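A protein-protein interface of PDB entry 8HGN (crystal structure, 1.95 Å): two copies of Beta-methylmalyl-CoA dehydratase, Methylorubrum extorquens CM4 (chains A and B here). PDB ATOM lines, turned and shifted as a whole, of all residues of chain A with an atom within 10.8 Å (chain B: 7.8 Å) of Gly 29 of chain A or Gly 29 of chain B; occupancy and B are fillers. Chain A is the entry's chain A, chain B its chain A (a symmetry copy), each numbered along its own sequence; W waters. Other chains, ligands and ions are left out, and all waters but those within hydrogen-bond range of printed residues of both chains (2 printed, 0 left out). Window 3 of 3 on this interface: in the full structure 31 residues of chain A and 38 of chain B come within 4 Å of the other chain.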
ATOM      1  N   ARG A  24      14.336  -1.848 -13.801  1.00  0.00           N
ATOM      2  CA  ARG A  24      15.365  -2.871 -13.567  1.00  0.00           C
ATOM      3  C   ARG A  24      16.275  -2.479 -12.414  1.00  0.00           C
ATOM      4  O   ARG A  24      17.021  -1.506 -12.607  1.00  0.00           O
ATOM      5  CB  ARG A  24      16.220  -3.033 -14.824  1.00  0.00           C
ATOM      6  CG  ARG A  24      17.207  -4.186 -14.721  1.00  0.00           C
ATOM      7  CD  ARG A  24      16.546  -5.527 -14.404  1.00  0.00           C
ATOM      8  NE  ARG A  24      17.311  -6.568 -15.099  1.00  0.00           N
ATOM      9  CZ  ARG A  24      18.409  -7.091 -14.628  1.00  0.00           C
ATOM     10  NH1 ARG A  24      18.817  -6.738 -13.418  1.00  0.00           N
ATOM     11  NH2 ARG A  24      19.058  -8.018 -15.313  1.00  0.00           N
ATOM     12  N   THR A  25      16.270  -3.267 -11.329  1.00  0.00           N
ATOM     13  CA  THR A  25      17.305  -3.211 -10.267  1.00  0.00           C
ATOM     14  C   THR A  25      18.571  -3.912 -10.772  1.00  0.00           C
ATOM     15  O   THR A  25      18.526  -5.108 -11.098  1.00  0.00           O
ATOM     16  CB  THR A  25      16.834  -3.796  -8.935  1.00  0.00           C
ATOM     17  OG1 THR A  25      15.527  -3.303  -8.666  1.00  0.00           O
ATOM     18  CG2 THR A  25      17.783  -3.449  -7.811  1.00  0.00           C
ATOM     19  N   VAL A  26      19.657  -3.161 -10.879  1.00  0.00           N
ATOM     20  CA  VAL A  26      20.959  -3.671 -11.345  1.00  0.00           C
ATOM     21  C   VAL A  26      21.740  -3.981 -10.073  1.00  0.00           C
ATOM     22  O   VAL A  26      21.713  -3.131  -9.140  1.00  0.00           O
ATOM     23  CB  VAL A  26      21.636  -2.693 -12.331  1.00  0.00           C
ATOM     24  CG1 VAL A  26      22.897  -3.282 -12.934  1.00  0.00           C
ATOM     25  CG2 VAL A  26      20.715  -2.242 -13.455  1.00  0.00           C
ATOM     26  N   THR A  27      22.237  -5.224  -9.980  1.00  0.00           N
ATOM     27  CA  THR A  27      22.922  -5.827  -8.817  1.00  0.00           C
ATOM     28  C   THR A  27      24.332  -6.235  -9.240  1.00  0.00           C
ATOM     29  O   THR A  27      24.682  -6.123 -10.467  1.00  0.00           O
ATOM     30  CB  THR A  27      22.143  -7.034  -8.279  1.00  0.00           C
ATOM     31  OG1 THR A  27      22.332  -8.132  -9.171  1.00  0.00           O
ATOM     32  CG2 THR A  27      20.652  -6.785  -8.140  1.00  0.00           C
ATOM     33  N   THR A  28      25.107  -6.754  -8.298  1.00  0.00           N
ATOM     34  CA  THR A  28      26.435  -7.370  -8.585  1.00  0.00           C
ATOM     35  C   THR A  28      26.261  -8.676  -9.388  1.00  0.00           C
ATOM     36  O   THR A  28      27.244  -9.092 -10.011  1.00  0.00           O
ATOM     37  CB  THR A  28      27.240  -7.542  -7.292  1.00  0.00           C
ATOM     38  OG1 THR A  28      26.430  -8.161  -6.308  1.00  0.00           O
ATOM     39  CG2 THR A  28      27.697  -6.218  -6.720  1.00  0.00           C
ATOM     40  N   GLY A  29      25.068  -9.287  -9.414  1.00  0.00           N
ATOM     41  CA  GLY A  29      24.761 -10.331 -10.427  1.00  0.00           C
ATOM     42  C   GLY A  29      25.007  -9.825 -11.843  1.00  0.00           C
ATOM     43  O   GLY A  29      25.713 -10.464 -12.625  1.00  0.00           O
ATOM     44  N   ASP A  30      24.453  -8.667 -12.188  1.00  0.00           N
ATOM     45  CA  ASP A  30      24.515  -8.101 -13.543  1.00  0.00           C
ATOM     46  C   ASP A  30      25.965  -7.746 -13.827  1.00  0.00           C
ATOM     47  O   ASP A  30      26.402  -7.991 -14.956  1.00  0.00           O
ATOM     48  CB  ASP A  30      23.560  -6.929 -13.670  1.00  0.00           C
ATOM     49  CG  ASP A  30      22.154  -7.353 -13.285  1.00  0.00           C
ATOM     50  OD1 ASP A  30      21.655  -8.354 -13.899  1.00  0.00           O
ATOM     51  OD2 ASP A  30      21.597  -6.769 -12.301  1.00  0.00           O
ATOM     52  N   VAL A  31      26.653  -7.141 -12.845  1.00  0.00           N
ATOM     53  CA  VAL A  31      28.084  -6.731 -12.999  1.00  0.00           C
ATOM     54  C   VAL A  31      28.916  -7.970 -13.351  1.00  0.00           C
ATOM     55  O   VAL A  31      29.806  -7.906 -14.229  1.00  0.00           O
ATOM     56  CB  VAL A  31      28.590  -6.042 -11.709  1.00  0.00           C
ATOM     57  CG1 VAL A  31      30.082  -5.903 -11.685  1.00  0.00           C
ATOM     58  CG2 VAL A  31      27.906  -4.712 -11.470  1.00  0.00           C
ATOM     59  N   ALA A  32      28.752  -9.052 -12.605  1.00  0.00           N
ATOM     60  CA  ALA A  32      29.539 -10.292 -12.829  1.00  0.00           C
ATOM     61  C   ALA A  32      29.219 -10.876 -14.226  1.00  0.00           C
ATOM     62  O   ALA A  32      30.122 -11.413 -14.894  1.00  0.00           O
ATOM     63  CB  ALA A  32      29.174 -11.284 -11.759  1.00  0.00           C
ATOM     64  N   LEU A  33      27.962 -10.815 -14.661  1.00  0.00           N
ATOM     65  CA  LEU A  33      27.577 -11.441 -15.976  1.00  0.00           C
ATOM     66  C   LEU A  33      28.076 -10.562 -17.123  1.00  0.00           C
ATOM     67  O   LEU A  33      28.614 -11.131 -18.170  1.00  0.00           O
ATOM     68  CB  LEU A  33      26.056 -11.676 -16.000  1.00  0.00           C
ATOM     69  CG  LEU A  33      25.530 -12.588 -17.107  1.00  0.00           C
ATOM     70  CD1 LEU A  33      26.232 -13.934 -17.124  1.00  0.00           C
ATOM     71  CD2 LEU A  33      24.036 -12.805 -16.985  1.00  0.00           C
ATOM     72  N   TYR A  34      27.965  -9.235 -16.952  1.00  0.00           N
ATOM     73  CA  TYR A  34      28.493  -8.228 -17.903  1.00  0.00           C
ATOM     74  C   TYR A  34      29.989  -8.495 -18.042  1.00  0.00           C
ATOM     75  O   TYR A  34      30.490  -8.486 -19.194  1.00  0.00           O
ATOM     76  CB  TYR A  34      28.195  -6.779 -17.465  1.00  0.00           C
ATOM     77  CG  TYR A  34      28.551  -5.772 -18.537  1.00  0.00           C
ATOM     78  CD1 TYR A  34      29.824  -5.223 -18.633  1.00  0.00           C
ATOM     79  CD2 TYR A  34      27.632  -5.432 -19.512  1.00  0.00           C
ATOM     80  CE1 TYR A  34      30.137  -4.312 -19.630  1.00  0.00           C
ATOM     81  CE2 TYR A  34      27.959  -4.589 -20.551  1.00  0.00           C
ATOM     82  CZ  TYR A  34      29.211  -4.029 -20.619  1.00  0.00           C
ATOM     83  OH  TYR A  34      29.471  -3.215 -21.679  1.00  0.00           O
ATOM     84  N   THR A  35      30.701  -8.721 -16.909  1.00  0.00           N
ATOM     85  CA  THR A  35      32.171  -8.968 -16.925  1.00  0.00           C
ATOM     86  C   THR A  35      32.479 -10.227 -17.759  1.00  0.00           C
ATOM     87  O   THR A  35      33.411 -10.191 -18.558  1.00  0.00           O
ATOM     88  CB  THR A  35      32.775  -9.060 -15.520  1.00  0.00           C
ATOM     89  OG1 THR A  35      32.442  -7.873 -14.791  1.00  0.00           O
ATOM     90  CG2 THR A  35      34.271  -9.309 -15.541  1.00  0.00           C
ATOM     91  N   ALA A  36      31.730 -11.290 -17.581  1.00  0.00           N
ATOM     92  CA  ALA A  36      31.904 -12.565 -18.299  1.00  0.00           C
ATOM     93  C   ALA A  36      31.398 -12.471 -19.760  1.00  0.00           C
ATOM     94  O   ALA A  36      31.914 -13.245 -20.582  1.00  0.00           O
ATOM     95  CB  ALA A  36      31.218 -13.655 -17.526  1.00  0.00           C
ATOM     96  N   LEU A  37      30.472 -11.564 -20.117  1.00  0.00           N
ATOM     97  CA  LEU A  37      29.948 -11.512 -21.518  1.00  0.00           C
ATOM     98  C   LEU A  37      30.913 -10.691 -22.419  1.00  0.00           C
ATOM     99  O   LEU A  37      31.115 -11.036 -23.653  1.00  0.00           O
ATOM    100  CB  LEU A  37      28.508 -11.016 -21.478  1.00  0.00           C
ATOM    101  CG  LEU A  37      27.472 -12.045 -21.010  1.00  0.00           C
ATOM    102  CD1 LEU A  37      26.177 -11.368 -20.626  1.00  0.00           C
ATOM    103  CD2 LEU A  37      27.205 -13.065 -22.080  1.00  0.00           C
ATOM    104  N   LEU A  61      28.577   1.074 -11.939  1.00  0.00           N
ATOM    105  CA  LEU A  61      28.252   0.172 -13.079  1.00  0.00           C
ATOM    106  C   LEU A  61      29.052   0.647 -14.286  1.00  0.00           C
ATOM    107  O   LEU A  61      29.158   1.863 -14.463  1.00  0.00           O
ATOM    108  CB  LEU A  61      26.751   0.196 -13.416  1.00  0.00           C
ATOM    109  CG  LEU A  61      25.763  -0.156 -12.309  1.00  0.00           C
ATOM    110  CD1 LEU A  61      24.371  -0.268 -12.907  1.00  0.00           C
ATOM    111  CD2 LEU A  61      26.116  -1.447 -11.570  1.00  0.00           C
ATOM    112  N   LEU A  65      26.780  -1.096 -19.269  1.00  0.00           N
ATOM    113  CA  LEU A  65      25.760  -1.937 -18.590  1.00  0.00           C
ATOM    114  C   LEU A  65      24.562  -1.020 -18.305  1.00  0.00           C
ATOM    115  O   LEU A  65      23.464  -1.421 -18.555  1.00  0.00           O
ATOM    116  CB  LEU A  65      26.352  -2.624 -17.355  1.00  0.00           C
ATOM    117  CG  LEU A  65      25.358  -3.233 -16.366  1.00  0.00           C
ATOM    118  CD1 LEU A  65      24.392  -4.178 -17.054  1.00  0.00           C
ATOM    119  CD2 LEU A  65      26.092  -3.930 -15.214  1.00  0.00           C
ATOM    120  N   VAL A  69      20.841  -1.587 -20.267  1.00  0.00           N
ATOM    121  CA  VAL A  69      19.622  -1.776 -19.428  1.00  0.00           C
ATOM    122  C   VAL A  69      18.577  -0.725 -19.784  1.00  0.00           C
ATOM    123  O   VAL A  69      17.398  -1.092 -19.855  1.00  0.00           O
ATOM    124  CB  VAL A  69      19.919  -1.790 -17.928  1.00  0.00           C
ATOM    125  CG1 VAL A  69      18.628  -1.805 -17.125  1.00  0.00           C
ATOM    126  CG2 VAL A  69      20.783  -2.975 -17.560  1.00  0.00           C
ATOM    127  N   TYR A  98      24.922   2.786  -9.245  1.00  0.00           N
ATOM    128  CA  TYR A  98      25.463   1.785  -8.295  1.00  0.00           C
ATOM    129  C   TYR A  98      24.525   0.596  -8.170  1.00  0.00           C
ATOM    130  O   TYR A  98      23.310   0.733  -8.274  1.00  0.00           O
ATOM    131  CB  TYR A  98      25.752   2.434  -6.933  1.00  0.00           C
ATOM    132  CG  TYR A  98      26.774   3.517  -7.104  1.00  0.00           C
ATOM    133  CD1 TYR A  98      28.077   3.189  -7.436  1.00  0.00           C
ATOM    134  CD2 TYR A  98      26.408   4.852  -7.116  1.00  0.00           C
ATOM    135  CE1 TYR A  98      29.012   4.170  -7.729  1.00  0.00           C
ATOM    136  CE2 TYR A  98      27.338   5.845  -7.384  1.00  0.00           C
ATOM    137  CZ  TYR A  98      28.644   5.503  -7.682  1.00  0.00           C
ATOM    138  OH  TYR A  98      29.567   6.467  -7.949  1.00  0.00           O
ATOM    139  N   PRO A  99      25.098  -0.591  -7.892  1.00  0.00           N
ATOM    140  CA  PRO A  99      24.328  -1.793  -7.598  1.00  0.00           C
ATOM    141  C   PRO A  99      23.261  -1.512  -6.547  1.00  0.00           C
ATOM    142  O   PRO A  99      23.594  -0.928  -5.540  1.00  0.00           O
ATOM    143  CB  PRO A  99      25.346  -2.793  -7.027  1.00  0.00           C
ATOM    144  CG  PRO A  99      26.681  -2.306  -7.538  1.00  0.00           C
ATOM    145  CD  PRO A  99      26.529  -0.855  -7.955  1.00  0.00           C
ATOM    146  N   GLY A 100      22.039  -1.957  -6.803  1.00  0.00           N
ATOM    147  CA  GLY A 100      20.907  -1.789  -5.881  1.00  0.00           C
ATOM    148  C   GLY A 100      19.956  -0.746  -6.428  1.00  0.00           C
ATOM    149  O   GLY A 100      18.791  -0.817  -6.081  1.00  0.00           O
ATOM    150  N   GLU A 101      20.445   0.149  -7.288  1.00  0.00           N
ATOM    151  CA  GLU A 101      19.657   1.244  -7.882  1.00  0.00           C
ATOM    152  C   GLU A 101      18.746   0.592  -8.917  1.00  0.00           C
ATOM    153  O   GLU A 101      19.119  -0.486  -9.429  1.00  0.00           O
ATOM    154  CB  GLU A 101      20.568   2.326  -8.464  1.00  0.00           C
ATOM    155  CG  GLU A 101      21.405   3.049  -7.405  1.00  0.00           C
ATOM    156  CD  GLU A 101      21.905   4.448  -7.763  1.00  0.00           C
ATOM    157  OE1 GLU A 101      21.263   5.417  -7.323  1.00  0.00           O
ATOM    158  OE2 GLU A 101      22.938   4.577  -8.471  1.00  0.00           O
ATOM    159  N   ILE A 219      22.243 -14.503 -24.220  1.00  0.00           N
ATOM    160  CA  ILE A 219      22.232 -14.441 -22.730  1.00  0.00           C
ATOM    161  C   ILE A 219      22.361 -12.947 -22.352  1.00  0.00           C
ATOM    162  O   ILE A 219      21.589 -12.464 -21.463  1.00  0.00           O
ATOM    163  CB  ILE A 219      23.330 -15.356 -22.131  1.00  0.00           C
ATOM    164  CG1 ILE A 219      22.879 -16.813 -22.040  1.00  0.00           C
ATOM    165  CG2 ILE A 219      23.827 -14.843 -20.781  1.00  0.00           C
ATOM    166  CD1 ILE A 219      24.025 -17.773 -21.734  1.00  0.00           C
ATOM    167  N   ALA A 220      23.226 -12.200 -23.068  1.00  0.00           N
ATOM    168  CA  ALA A 220      23.455 -10.751 -22.867  1.00  0.00           C
ATOM    169  C   ALA A 220      22.157 -10.002 -23.151  1.00  0.00           C
ATOM    170  O   ALA A 220      21.810  -9.085 -22.387  1.00  0.00           O
ATOM    171  CB  ALA A 220      24.542 -10.259 -23.798  1.00  0.00           C
ATOM    172  N   LEU A 223      19.573 -10.492 -20.584  1.00  0.00           N
ATOM    173  CA  LEU A 223      19.983  -9.801 -19.323  1.00  0.00           C
ATOM    174  C   LEU A 223      19.448  -8.366 -19.339  1.00  0.00           C
ATOM    175  O   LEU A 223      19.086  -7.845 -18.259  1.00  0.00           O
ATOM    176  CB  LEU A 223      21.509  -9.786 -19.222  1.00  0.00           C
ATOM    177  CG  LEU A 223      22.069  -9.261 -17.906  1.00  0.00           C
ATOM    178  CD1 LEU A 223      21.604 -10.110 -16.723  1.00  0.00           C
ATOM    179  CD2 LEU A 223      23.602  -9.154 -17.976  1.00  0.00           C
ATOM    180  N   PHE A 224      19.516  -7.700 -20.506  1.00  0.00           N
ATOM    181  CA  PHE A 224      19.095  -6.293 -20.713  1.00  0.00           C
ATOM    182  C   PHE A 224      17.562  -6.263 -20.816  1.00  0.00           C
ATOM    183  O   PHE A 224      16.934  -5.189 -20.906  1.00  0.00           O
ATOM    184  CB  PHE A 224      19.813  -5.734 -21.948  1.00  0.00           C
ATOM    185  CG  PHE A 224      21.315  -5.863 -21.923  1.00  0.00           C
ATOM    186  CD1 PHE A 224      22.030  -5.711 -20.745  1.00  0.00           C
ATOM    187  CD2 PHE A 224      22.010  -6.216 -23.059  1.00  0.00           C
ATOM    188  CE1 PHE A 224      23.408  -5.846 -20.737  1.00  0.00           C
ATOM    189  CE2 PHE A 224      23.388  -6.338 -23.050  1.00  0.00           C
ATOM    190  CZ  PHE A 224      24.085  -6.131 -21.897  1.00  0.00           C
ATOM    191  N   ARG B  24      21.061 -24.741  -0.735  1.00  0.00           N
ATOM    192  CA  ARG B  24      21.457 -23.692  -1.685  1.00  0.00           C
ATOM    193  C   ARG B  24      21.065 -22.315  -1.175  1.00  0.00           C
ATOM    194  O   ARG B  24      19.848 -22.072  -1.124  1.00  0.00           O
ATOM    195  CB  ARG B  24      20.758 -23.927  -3.025  1.00  0.00           C
ATOM    196  CG  ARG B  24      21.237 -22.978  -4.114  1.00  0.00           C
ATOM    197  CD  ARG B  24      22.748 -23.019  -4.336  1.00  0.00           C
ATOM    198  NE  ARG B  24      22.986 -22.794  -5.766  1.00  0.00           N
ATOM    199  CZ  ARG B  24      23.021 -21.610  -6.314  1.00  0.00           C
ATOM    200  NH1 ARG B  24      22.926 -20.544  -5.534  1.00  0.00           N
ATOM    201  NH2 ARG B  24      23.228 -21.478  -7.614  1.00  0.00           N
ATOM    202  N   VAL B  26      20.446 -18.757  -2.278  1.00  0.00           N
ATOM    203  CA  VAL B  26      20.065 -18.077  -3.529  1.00  0.00           C
ATOM    204  C   VAL B  26      20.344 -16.599  -3.275  1.00  0.00           C
ATOM    205  O   VAL B  26      19.972 -16.108  -2.173  1.00  0.00           O
ATOM    206  CB  VAL B  26      18.622 -18.429  -3.955  1.00  0.00           C
ATOM    207  CG1 VAL B  26      18.281 -17.860  -5.318  1.00  0.00           C
ATOM    208  CG2 VAL B  26      18.348 -19.926  -3.961  1.00  0.00           C
ATOM    209  N   THR B  27      21.131 -15.990  -4.173  1.00  0.00           N
ATOM    210  CA  THR B  27      21.658 -14.610  -4.109  1.00  0.00           C
ATOM    211  C   THR B  27      21.156 -13.840  -5.328  1.00  0.00           C
ATOM    212  O   THR B  27      20.495 -14.455  -6.237  1.00  0.00           O
ATOM    213  CB  THR B  27      23.191 -14.602  -4.052  1.00  0.00           C
ATOM    214  OG1 THR B  27      23.696 -14.912  -5.351  1.00  0.00           O
ATOM    215  CG2 THR B  27      23.770 -15.601  -3.067  1.00  0.00           C
ATOM    216  N   THR B  28      21.498 -12.561  -5.404  1.00  0.00           N
ATOM    217  CA  THR B  28      21.249 -11.722  -6.613  1.00  0.00           C
ATOM    218  C   THR B  28      22.129 -12.195  -7.788  1.00  0.00           C
ATOM    219  O   THR B  28      21.778 -11.864  -8.926  1.00  0.00           O
ATOM    220  CB  THR B  28      21.409 -10.235  -6.280  1.00  0.00           C
ATOM    221  OG1 THR B  28      22.626 -10.035  -5.583  1.00  0.00           O
ATOM    222  CG2 THR B  28      20.301  -9.723  -5.387  1.00  0.00           C
ATOM    223  N   GLY B  29      23.201 -12.963  -7.549  1.00  0.00           N
ATOM    224  CA  GLY B  29      23.868 -13.715  -8.646  1.00  0.00           C
ATOM    225  C   GLY B  29      22.879 -14.595  -9.400  1.00  0.00           C
ATOM    226  O   GLY B  29      22.794 -14.535 -10.627  1.00  0.00           O
ATOM    227  N   ASP B  30      22.105 -15.405  -8.685  1.00  0.00           N
ATOM    228  CA  ASP B  30      21.178 -16.383  -9.273  1.00  0.00           C
ATOM    229  C   ASP B  30      20.085 -15.608  -9.989  1.00  0.00           C
ATOM    230  O   ASP B  30      19.702 -16.037 -11.081  1.00  0.00           O
ATOM    231  CB  ASP B  30      20.662 -17.329  -8.205  1.00  0.00           C
ATOM    232  CG  ASP B  30      21.821 -17.993  -7.486  1.00  0.00           C
ATOM    233  OD1 ASP B  30      22.677 -18.614  -8.201  1.00  0.00           O
ATOM    234  OD2 ASP B  30      21.943 -17.801  -6.234  1.00  0.00           O
ATOM    235  N   VAL B  31      19.575 -14.538  -9.356  1.00  0.00           N
ATOM    236  CA  VAL B  31      18.490 -13.695  -9.946  1.00  0.00           C
ATOM    237  C   VAL B  31      18.965 -13.156 -11.300  1.00  0.00           C
ATOM    238  O   VAL B  31      18.191 -13.140 -12.283  1.00  0.00           O
ATOM    239  CB  VAL B  31      18.102 -12.556  -8.973  1.00  0.00           C
ATOM    240  CG1 VAL B  31      17.262 -11.504  -9.634  1.00  0.00           C
ATOM    241  CG2 VAL B  31      17.442 -13.082  -7.716  1.00  0.00           C
ATOM    242  N   ALA B  32      20.163 -12.589 -11.349  1.00  0.00           N
ATOM    243  CA  ALA B  32      20.703 -11.993 -12.598  1.00  0.00           C
ATOM    244  C   ALA B  32      20.881 -13.091 -13.674  1.00  0.00           C
ATOM    245  O   ALA B  32      20.654 -12.828 -14.869  1.00  0.00           O
ATOM    246  CB  ALA B  32      22.032 -11.360 -12.284  1.00  0.00           C
ATOM    247  N   LEU B  33      21.310 -14.290 -13.285  1.00  0.00           N
ATOM    248  CA  LEU B  33      21.579 -15.371 -14.299  1.00  0.00           C
ATOM    249  C   LEU B  33      20.251 -15.944 -14.796  1.00  0.00           C
ATOM    250  O   LEU B  33      20.107 -16.196 -16.071  1.00  0.00           O
ATOM    251  CB  LEU B  33      22.510 -16.428 -13.679  1.00  0.00           C
ATOM    252  CG  LEU B  33      23.148 -17.420 -14.650  1.00  0.00           C
ATOM    253  CD1 LEU B  33      23.883 -16.725 -15.782  1.00  0.00           C
ATOM    254  CD2 LEU B  33      24.099 -18.361 -13.938  1.00  0.00           C
ATOM    255  N   TYR B  34      19.290 -16.112 -13.874  1.00  0.00           N
ATOM    256  CA  TYR B  34      17.908 -16.550 -14.185  1.00  0.00           C
ATOM    257  C   TYR B  34      17.342 -15.545 -15.184  1.00  0.00           C
ATOM    258  O   TYR B  34      16.715 -15.985 -16.179  1.00  0.00           O
ATOM    259  CB  TYR B  34      17.027 -16.684 -12.926  1.00  0.00           C
ATOM    260  CG  TYR B  34      15.691 -17.329 -13.229  1.00  0.00           C
ATOM    261  CD1 TYR B  34      14.589 -16.578 -13.623  1.00  0.00           C
ATOM    262  CD2 TYR B  34      15.553 -18.703 -13.203  1.00  0.00           C
ATOM    263  CE1 TYR B  34      13.377 -17.185 -13.909  1.00  0.00           C
ATOM    264  CE2 TYR B  34      14.374 -19.319 -13.562  1.00  0.00           C
ATOM    265  CZ  TYR B  34      13.284 -18.566 -13.921  1.00  0.00           C
ATOM    266  OH  TYR B  34      12.155 -19.240 -14.277  1.00  0.00           O
ATOM    267  N   THR B  35      17.540 -14.225 -14.938  1.00  0.00           N
ATOM    268  CA  THR B  35      17.011 -13.157 -15.832  1.00  0.00           C
ATOM    269  C   THR B  35      17.605 -13.317 -17.245  1.00  0.00           C
ATOM    270  O   THR B  35      16.858 -13.214 -18.214  1.00  0.00           O
ATOM    271  CB  THR B  35      17.242 -11.747 -15.278  1.00  0.00           C
ATOM    272  OG1 THR B  35      16.684 -11.665 -13.963  1.00  0.00           O
ATOM    273  CG2 THR B  35      16.699 -10.664 -16.191  1.00  0.00           C
ATOM    274  N   LEU B  65      12.550 -19.814 -10.148  1.00  0.00           N
ATOM    275  CA  LEU B  65      13.953 -19.938  -9.669  1.00  0.00           C
ATOM    276  C   LEU B  65      13.894 -20.732  -8.358  1.00  0.00           C
ATOM    277  O   LEU B  65      14.678 -21.620  -8.192  1.00  0.00           O
ATOM    278  CB  LEU B  65      14.615 -18.561  -9.559  1.00  0.00           C
ATOM    279  CG  LEU B  65      15.917 -18.489  -8.761  1.00  0.00           C
ATOM    280  CD1 LEU B  65      16.934 -19.500  -9.256  1.00  0.00           C
ATOM    281  CD2 LEU B  65      16.492 -17.067  -8.782  1.00  0.00           C
ATOM    282  N   PRO B  99      16.656 -13.247  -1.631  1.00  0.00           N
ATOM    283  CA  PRO B  99      18.102 -13.403  -1.735  1.00  0.00           C
ATOM    284  C   PRO B  99      18.741 -13.477  -0.353  1.00  0.00           C
ATOM    285  O   PRO B  99      18.431 -12.640   0.464  1.00  0.00           O
ATOM    286  CB  PRO B  99      18.593 -12.133  -2.449  1.00  0.00           C
ATOM    287  CG  PRO B  99      17.377 -11.615  -3.178  1.00  0.00           C
ATOM    288  CD  PRO B  99      16.144 -12.236  -2.546  1.00  0.00           C
ATOM    289  N   LEU B 223      23.264 -24.360 -12.699  1.00  0.00           N
ATOM    290  CA  LEU B 223      22.912 -23.309 -11.696  1.00  0.00           C
ATOM    291  C   LEU B 223      22.011 -23.922 -10.619  1.00  0.00           C
ATOM    292  O   LEU B 223      22.120 -23.515  -9.440  1.00  0.00           O
ATOM    293  CB  LEU B 223      22.181 -22.161 -12.394  1.00  0.00           C
ATOM    294  CG  LEU B 223      21.907 -20.940 -11.525  1.00  0.00           C
ATOM    295  CD1 LEU B 223      23.206 -20.322 -11.005  1.00  0.00           C
ATOM    296  CD2 LEU B 223      21.042 -19.919 -12.285  1.00  0.00           C
HETATM  297  O   HOH W   1      19.852  -9.291 -10.576  1.00  0.00           O
HETATM  298  O   HOH W   2      23.646  -7.953  -4.237  1.00  0.00           O
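The guanidinium group (NH2) of Arg 24 of chain A is in salt-bridge range of the side-chain carboxylate (OD1) of Asp 30 of chain A.
O of Leu 223 of chain A sits at hydrogen-bond distance from NH2 of Arg 24 of chain A, 3.0 Å away.
N of Gly 29 of chain A is in hydrogen-bond range of OG1 of Thr 27 of chain A, at 3.0 Å.
The side-chain carboxylate of Asp 30 of chain A sits at hydrogen-bond distance from the backbone NH of Thr 27 of chain A (2.9 Å).
OG1 of Thr 27 of chain B lies within hydrogen-bond range of N of Gly 29 of chain B (3.0 Å).
The side-chain hydroxyl (OG1) of Thr 35 of chain B is in hydrogen-bond range of the backbone carbonyl oxygen (O) of Val 31 of chain B, at 2.7 Å.
Among the printed residues, pairs that only touch across the chains: Arg 24 of chain A with Thr 35 of chain B (3.7 Å), Thr 27 of chain A with Thr 28 of chain B (3.7 Å), Gly 29 of chain A with Thr 28 of chain B (3.7 Å), Gly 29 of chain A with Gly 29 of chain B (3.9 Å), Gly 29 of chain A with Ala 32 of chain B (3.4 Å), Asp 30 of chain A with Ala 32 of chain B (3.4 Å), Leu 33 of chain A with Ala 32 of chain B (3.99 Å), Leu 33 of chain A with Leu 33 of chain B (3.9 Å) and Leu 223 of chain A with Ala 32 of chain B (3.4 Å).
Printed residues of chain B within 4 Å of Gly 29 of chain A: Thr 28, Gly 29 and Ala 32.
Printed residues of chain B within 4 Å of Asp 30 of chain A: Ala 32.
Of the printed residues of chain B, Leu 33 of chain A touches Ala 32 and Leu 33.
Of the printed residues of chain B, Leu 223 of chain A touches Ala 32.
No residue of chain A comes within 4 Å of Thr 27 of chain B.
Thr 28 of chain B touches just these residues of chain A: Thr 27 and Gly 29.
Gly 29 of chain B touches one residue of chain A.
No residue of chain A comes within 4 Å of Asp 30 of chain B.
No residue of chain A comes within 4 Å of Val 31 of chain B.
Printed residues of chain A within 4 Å of Leu 33 of chain B: Leu 33.
Printed residues of chain A within 4 Å of Thr 35 of chain B: Arg 24.
The nearest printed residue of chain A that does not touch Ala 32 of chain B is Thr 27 of chain A (4.5 Å).
Of the 25 printed residues of chain A, 6 touch a printed residue of chain B.
Printed residues of chain A that touch a printed residue of chain B: Arg 24, Thr 27, Gly 29, Asp 30, Leu 33 and Leu 223.
Hydrophobic or aromatic side chains of chain A that line the printed part of chain B: Leu 33 and Leu 223.
Among the printed residues, no Asp or Glu carboxylate lies within 4 Å of a Lys or Arg side-chain nitrogen of the other chain.
Gly 29 of chain A touches Thr 28 of chain B, but with the chains exchanged Thr 28 of chain A does not touch Gly 29 of chain B (5.6 Å).
Gly 29 of chain A touches Ala 32 of chain B, but with the chains exchanged Ala 32 of chain A does not touch Gly 29 of chain B (6.6 Å).
Leu 33 of chain A touches its own counterpart, Leu 33 of chain B.
Leu 223 of chain A touches Ala 32 of chain B, but with the chains exchanged Ala 32 of chain A does not touch Leu 223 of chain B (10.9 Å).
14 positions are printed for both chains.
Of the 9 pairs that touch across the chains among the printed residues, 2 have their exchanged pair printed and touching as well.
Water W2 lies within hydrogen-bond range of OG1 of Thr 28 of chain B (2.7 Å) and OG1 of Thr 28 of chain A (3.5 Å).
Water W1 bridges the side-chain hydroxyl of Thr 27 of chain A and the backbone NH of Ala 32 of chain B.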
